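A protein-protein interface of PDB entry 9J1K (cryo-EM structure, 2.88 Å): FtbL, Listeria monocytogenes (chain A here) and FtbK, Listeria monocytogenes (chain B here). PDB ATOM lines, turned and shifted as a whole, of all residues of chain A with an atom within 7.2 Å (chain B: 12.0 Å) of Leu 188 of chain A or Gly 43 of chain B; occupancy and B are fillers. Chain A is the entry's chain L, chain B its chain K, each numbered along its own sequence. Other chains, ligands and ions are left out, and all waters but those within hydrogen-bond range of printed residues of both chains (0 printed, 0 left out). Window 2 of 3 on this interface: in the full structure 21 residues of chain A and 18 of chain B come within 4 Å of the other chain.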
ATOM      1  N   ARG A 186       4.397 -19.541   6.627  1.00  0.00           N
ATOM      2  CA  ARG A 186       5.160 -18.491   5.973  1.00  0.00           C
ATOM      3  C   ARG A 186       6.646 -18.690   6.223  1.00  0.00           C
ATOM      4  O   ARG A 186       7.063 -19.007   7.341  1.00  0.00           O
ATOM      5  CB  ARG A 186       4.729 -17.108   6.459  1.00  0.00           C
ATOM      6  CG  ARG A 186       3.508 -16.568   5.741  1.00  0.00           C
ATOM      7  CD  ARG A 186       3.890 -15.482   4.756  1.00  0.00           C
ATOM      8  NE  ARG A 186       2.725 -14.774   4.244  1.00  0.00           N
ATOM      9  CZ  ARG A 186       2.703 -14.098   3.105  1.00  0.00           C
ATOM     10  NH1 ARG A 186       3.771 -14.018   2.329  1.00  0.00           N
ATOM     11  NH2 ARG A 186       1.583 -13.486   2.735  1.00  0.00           N
ATOM     12  N   TYR A 187       7.437 -18.503   5.171  1.00  0.00           N
ATOM     13  CA  TYR A 187       8.881 -18.644   5.277  1.00  0.00           C
ATOM     14  C   TYR A 187       9.461 -17.512   6.114  1.00  0.00           C
ATOM     15  O   TYR A 187       9.034 -16.358   6.006  1.00  0.00           O
ATOM     16  CB  TYR A 187       9.500 -18.668   3.879  1.00  0.00           C
ATOM     17  CG  TYR A 187      10.886 -18.080   3.766  1.00  0.00           C
ATOM     18  CD1 TYR A 187      12.000 -18.797   4.176  1.00  0.00           C
ATOM     19  CD2 TYR A 187      11.082 -16.820   3.220  1.00  0.00           C
ATOM     20  CE1 TYR A 187      13.271 -18.269   4.062  1.00  0.00           C
ATOM     21  CE2 TYR A 187      12.348 -16.283   3.102  1.00  0.00           C
ATOM     22  CZ  TYR A 187      13.438 -17.013   3.522  1.00  0.00           C
ATOM     23  OH  TYR A 187      14.701 -16.480   3.409  1.00  0.00           O
ATOM     24  N   LEU A 188      10.413 -17.864   6.983  1.00  0.00           N
ATOM     25  CA  LEU A 188      11.103 -16.940   7.881  1.00  0.00           C
ATOM     26  C   LEU A 188      10.206 -16.422   9.000  1.00  0.00           C
ATOM     27  O   LEU A 188      10.676 -15.696   9.882  1.00  0.00           O
ATOM     28  CB  LEU A 188      11.692 -15.753   7.112  1.00  0.00           C
ATOM     29  CG  LEU A 188      13.156 -15.836   6.691  1.00  0.00           C
ATOM     30  CD1 LEU A 188      13.583 -14.543   6.020  1.00  0.00           C
ATOM     31  CD2 LEU A 188      14.041 -16.140   7.884  1.00  0.00           C
ATOM     32  N   TYR A 189       8.924 -16.783   8.990  1.00  0.00           N
ATOM     33  CA  TYR A 189       7.998 -16.324  10.020  1.00  0.00           C
ATOM     34  C   TYR A 189       7.752 -17.386  11.087  1.00  0.00           C
ATOM     35  O   TYR A 189       7.985 -17.143  12.274  1.00  0.00           O
ATOM     36  CB  TYR A 189       6.666 -15.895   9.394  1.00  0.00           C
ATOM     37  CG  TYR A 189       5.673 -15.395  10.414  1.00  0.00           C
ATOM     38  CD1 TYR A 189       5.870 -14.187  11.068  1.00  0.00           C
ATOM     39  CD2 TYR A 189       4.551 -16.140  10.740  1.00  0.00           C
ATOM     40  CE1 TYR A 189       4.969 -13.729  12.006  1.00  0.00           C
ATOM     41  CE2 TYR A 189       3.645 -15.691  11.678  1.00  0.00           C
ATOM     42  CZ  TYR A 189       3.858 -14.485  12.308  1.00  0.00           C
ATOM     43  OH  TYR A 189       2.958 -14.033  13.243  1.00  0.00           O
ATOM     44  N   ASN A 190       7.284 -18.566  10.683  1.00  0.00           N
ATOM     45  CA  ASN A 190       6.972 -19.631  11.626  1.00  0.00           C
ATOM     46  C   ASN A 190       7.486 -20.989  11.169  1.00  0.00           C
ATOM     47  O   ASN A 190       7.073 -22.012  11.726  1.00  0.00           O
ATOM     48  CB  ASN A 190       5.461 -19.704  11.874  1.00  0.00           C
ATOM     49  CG  ASN A 190       4.661 -19.669  10.590  1.00  0.00           C
ATOM     50  OD1 ASN A 190       5.221 -19.686   9.496  1.00  0.00           O
ATOM     51  ND2 ASN A 190       3.341 -19.621  10.718  1.00  0.00           N
ATOM     52  N   THR A 191       8.369 -21.030  10.177  1.00  0.00           N
ATOM     53  CA  THR A 191       8.956 -22.274   9.706  1.00  0.00           C
ATOM     54  C   THR A 191      10.472 -22.155   9.722  1.00  0.00           C
ATOM     55  O   THR A 191      11.030 -21.071   9.533  1.00  0.00           O
ATOM     56  CB  THR A 191       8.458 -22.640   8.297  1.00  0.00           C
ATOM     57  OG1 THR A 191       8.841 -23.985   7.987  1.00  0.00           O
ATOM     58  CG2 THR A 191       9.030 -21.700   7.253  1.00  0.00           C
ATOM     59  N   GLU A 192      11.137 -23.280   9.978  1.00  0.00           N
ATOM     60  CA  GLU A 192      12.592 -23.307  10.085  1.00  0.00           C
ATOM     61  C   GLU A 192      13.232 -24.134   8.979  1.00  0.00           C
ATOM     62  O   GLU A 192      14.077 -23.617   8.242  1.00  0.00           O
ATOM     63  CB  GLU A 192      13.005 -23.837  11.464  1.00  0.00           C
ATOM     64  CG  GLU A 192      14.406 -24.420  11.516  1.00  0.00           C
ATOM     65  CD  GLU A 192      15.480 -23.353  11.554  1.00  0.00           C
ATOM     66  OE1 GLU A 192      15.841 -22.912  12.665  1.00  0.00           O
ATOM     67  OE2 GLU A 192      15.962 -22.953  10.474  1.00  0.00           O
ATOM     68  N   ILE A 294       3.405 -20.542   1.777  1.00  0.00           N
ATOM     69  CA  ILE A 294       4.102 -19.540   0.981  1.00  0.00           C
ATOM     70  C   ILE A 294       5.578 -19.602   1.346  1.00  0.00           C
ATOM     71  O   ILE A 294       5.944 -19.372   2.504  1.00  0.00           O
ATOM     72  CB  ILE A 294       3.550 -18.125   1.215  1.00  0.00           C
ATOM     73  CG1 ILE A 294       2.095 -18.033   0.759  1.00  0.00           C
ATOM     74  CG2 ILE A 294       4.402 -17.098   0.490  1.00  0.00           C
ATOM     75  CD1 ILE A 294       1.274 -17.057   1.563  1.00  0.00           C
ATOM     76  N   HIS A 295       6.419 -19.910   0.361  1.00  0.00           N
ATOM     77  CA  HIS A 295       7.863 -20.038   0.557  1.00  0.00           C
ATOM     78  C   HIS A 295       8.519 -19.639  -0.766  1.00  0.00           C
ATOM     79  O   HIS A 295       8.656 -20.457  -1.678  1.00  0.00           O
ATOM     80  CB  HIS A 295       8.236 -21.452   0.975  1.00  0.00           C
ATOM     81  CG  HIS A 295       9.563 -21.553   1.656  1.00  0.00           C
ATOM     82  ND1 HIS A 295       9.692 -21.884   2.988  1.00  0.00           N
ATOM     83  CD2 HIS A 295      10.821 -21.380   1.188  1.00  0.00           C
ATOM     84  CE1 HIS A 295      10.972 -21.903   3.313  1.00  0.00           C
ATOM     85  NE2 HIS A 295      11.679 -21.600   2.239  1.00  0.00           N
ATOM     86  N   GLU A 296       8.909 -18.367  -0.858  1.00  0.00           N
ATOM     87  CA  GLU A 296       9.429 -17.835  -2.116  1.00  0.00           C
ATOM     88  C   GLU A 296      10.718 -18.507  -2.576  1.00  0.00           C
ATOM     89  O   GLU A 296      10.805 -18.861  -3.765  1.00  0.00           O
ATOM     90  CB  GLU A 296       9.606 -16.317  -1.997  1.00  0.00           C
ATOM     91  CG  GLU A 296       8.355 -15.579  -1.547  1.00  0.00           C
ATOM     92  CD  GLU A 296       8.261 -15.453  -0.039  1.00  0.00           C
ATOM     93  OE1 GLU A 296       9.172 -15.948   0.657  1.00  0.00           O
ATOM     94  OE2 GLU A 296       7.275 -14.863   0.449  1.00  0.00           O
ATOM     95  N   ALA B  39      14.481 -20.506  21.160  1.00  0.00           N
ATOM     96  CA  ALA B  39      14.304 -21.209  19.898  1.00  0.00           C
ATOM     97  C   ALA B  39      14.744 -20.281  18.778  1.00  0.00           C
ATOM     98  O   ALA B  39      14.288 -19.135  18.706  1.00  0.00           O
ATOM     99  CB  ALA B  39      12.852 -21.648  19.696  1.00  0.00           C
ATOM    100  N   GLU B  40      15.623 -20.771  17.912  1.00  0.00           N
ATOM    101  CA  GLU B  40      16.217 -19.964  16.856  1.00  0.00           C
ATOM    102  C   GLU B  40      15.658 -20.381  15.505  1.00  0.00           C
ATOM    103  O   GLU B  40      15.605 -21.575  15.192  1.00  0.00           O
ATOM    104  CB  GLU B  40      17.741 -20.099  16.855  1.00  0.00           C
ATOM    105  CG  GLU B  40      18.474 -18.857  17.326  1.00  0.00           C
ATOM    106  CD  GLU B  40      19.751 -19.182  18.075  1.00  0.00           C
ATOM    107  OE1 GLU B  40      20.007 -20.379  18.321  1.00  0.00           O
ATOM    108  OE2 GLU B  40      20.497 -18.241  18.419  1.00  0.00           O
ATOM    109  N   ILE B  41      15.244 -19.398  14.714  1.00  0.00           N
ATOM    110  CA  ILE B  41      14.850 -19.603  13.326  1.00  0.00           C
ATOM    111  C   ILE B  41      15.924 -18.973  12.453  1.00  0.00           C
ATOM    112  O   ILE B  41      16.176 -17.765  12.545  1.00  0.00           O
ATOM    113  CB  ILE B  41      13.469 -19.004  13.027  1.00  0.00           C
ATOM    114  CG1 ILE B  41      12.383 -19.762  13.791  1.00  0.00           C
ATOM    115  CG2 ILE B  41      13.191 -19.032  11.535  1.00  0.00           C
ATOM    116  CD1 ILE B  41      10.988 -19.245  13.534  1.00  0.00           C
ATOM    117  N   ALA B  42      16.561 -19.790  11.617  1.00  0.00           N
ATOM    118  CA  ALA B  42      17.669 -19.311  10.804  1.00  0.00           C
ATOM    119  C   ALA B  42      17.208 -18.214   9.854  1.00  0.00           C
ATOM    120  O   ALA B  42      16.140 -18.303   9.245  1.00  0.00           O
ATOM    121  CB  ALA B  42      18.286 -20.467  10.019  1.00  0.00           C
ATOM    122  N   GLY B  43      18.027 -17.171   9.734  1.00  0.00           N
ATOM    123  CA  GLY B  43      17.719 -16.035   8.899  1.00  0.00           C
ATOM    124  C   GLY B  43      17.064 -14.874   9.618  1.00  0.00           C
ATOM    125  O   GLY B  43      17.084 -13.753   9.097  1.00  0.00           O
ATOM    126  N   THR B  44      16.492 -15.106  10.793  1.00  0.00           N
ATOM    127  CA  THR B  44      15.861 -14.057  11.578  1.00  0.00           C
ATOM    128  C   THR B  44      16.799 -13.580  12.680  1.00  0.00           C
ATOM    129  O   THR B  44      17.842 -14.177  12.951  1.00  0.00           O
ATOM    130  CB  THR B  44      14.542 -14.550  12.180  1.00  0.00           C
ATOM    131  OG1 THR B  44      14.698 -15.900  12.634  1.00  0.00           O
ATOM    132  CG2 THR B  44      13.434 -14.491  11.144  1.00  0.00           C
ATOM    133  N   ASP B  45      16.407 -12.487  13.325  1.00  0.00           N
ATOM    134  CA  ASP B  45      17.218 -11.855  14.354  1.00  0.00           C
ATOM    135  C   ASP B  45      16.778 -12.314  15.735  1.00  0.00           C
ATOM    136  O   ASP B  45      15.581 -12.426  16.013  1.00  0.00           O
ATOM    137  CB  ASP B  45      17.123 -10.333  14.264  1.00  0.00           C
ATOM    138  CG  ASP B  45      17.562  -9.805  12.920  1.00  0.00           C
ATOM    139  OD1 ASP B  45      18.729 -10.038  12.541  1.00  0.00           O
ATOM    140  OD2 ASP B  45      16.743  -9.155  12.239  1.00  0.00           O
ATOM    141  N   GLY B  46      17.755 -12.575  16.597  1.00  0.00           N
ATOM    142  CA  GLY B  46      17.450 -12.933  17.961  1.00  0.00           C
ATOM    143  C   GLY B  46      16.845 -14.322  18.087  1.00  0.00           C
ATOM    144  O   GLY B  46      17.008 -15.194  17.230  1.00  0.00           O
ATOM    145  N   VAL B  47      16.127 -14.513  19.193  1.00  0.00           N
ATOM    146  CA  VAL B  47      15.527 -15.793  19.534  1.00  0.00           C
ATOM    147  C   VAL B  47      14.076 -15.568  19.933  1.00  0.00           C
ATOM    148  O   VAL B  47      13.655 -14.450  20.238  1.00  0.00           O
ATOM    149  CB  VAL B  47      16.285 -16.507  20.673  1.00  0.00           C
ATOM    150  CG1 VAL B  47      17.701 -16.841  20.245  1.00  0.00           C
ATOM    151  CG2 VAL B  47      16.293 -15.639  21.917  1.00  0.00           C
ATOM    152  N   ILE B  48      13.311 -16.655  19.927  1.00  0.00           N
ATOM    153  CA  ILE B  48      11.932 -16.652  20.403  1.00  0.00           C
ATOM    154  C   ILE B  48      11.929 -17.291  21.792  1.00  0.00           C
ATOM    155  O   ILE B  48      12.117 -18.514  21.895  1.00  0.00           O
ATOM    156  CB  ILE B  48      10.998 -17.403  19.448  1.00  0.00           C
ATOM    157  CG1 ILE B  48      11.567 -17.395  18.030  1.00  0.00           C
ATOM    158  CG2 ILE B  48       9.609 -16.788  19.473  1.00  0.00           C
ATOM    159  CD1 ILE B  48      10.784 -18.245  17.062  1.00  0.00           C
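N of Ala 42 of chain B sits at hydrogen-bond distance from OE1 of Glu 192 of chain A, at 3.4 Å. The side-chain carboxylate of Glu 192 of chain A sits close to the backbone carbonyl oxygen of Glu 40 of chain B.
Among the printed residues, merely in contact across the chains: Leu 188 of chain A with Ala 42 of chain B, Leu 188 of chain A with Gly 43 of chain B, Leu 188 of chain A with Thr 44 of chain B, Tyr 189 of chain A with Ile 41 of chain B, Thr 191 of chain A with Ile 41 of chain B and Glu 192 of chain A with Ile 41 of chain B.
No residue of chain B comes within 4 Å of Tyr 187 of chain A. Leu 188 of chain A touches three residues of chain B. No residue of chain B comes within 4 Å of Asn 190 of chain A. Thr 191 of chain A touches just one residue of chain B: Ile 41 (3.6 Å). Of the printed residues of chain A, Glu 40 of chain B touches Glu 192 (2.9 Å). Gly 43 of chain B touches just one residue of chain A: Leu 188. Of the printed residues of chain A, Thr 44 of chain B touches Leu 188 (3.3 Å). The nearest residue of chain B that does not touch Leu 188 of chain A is Ile 41 of chain B (4.5 Å). The nearest printed residue of chain A that does not touch Ile 41 of chain B is Asn 190 of chain A (4.5 Å).
Among the printed residues, 8 pairs touch across the chains. Among the printed residues, no Asp or Glu carboxylate lies within 4 Å of a Lys or Arg side-chain nitrogen of the other chain.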
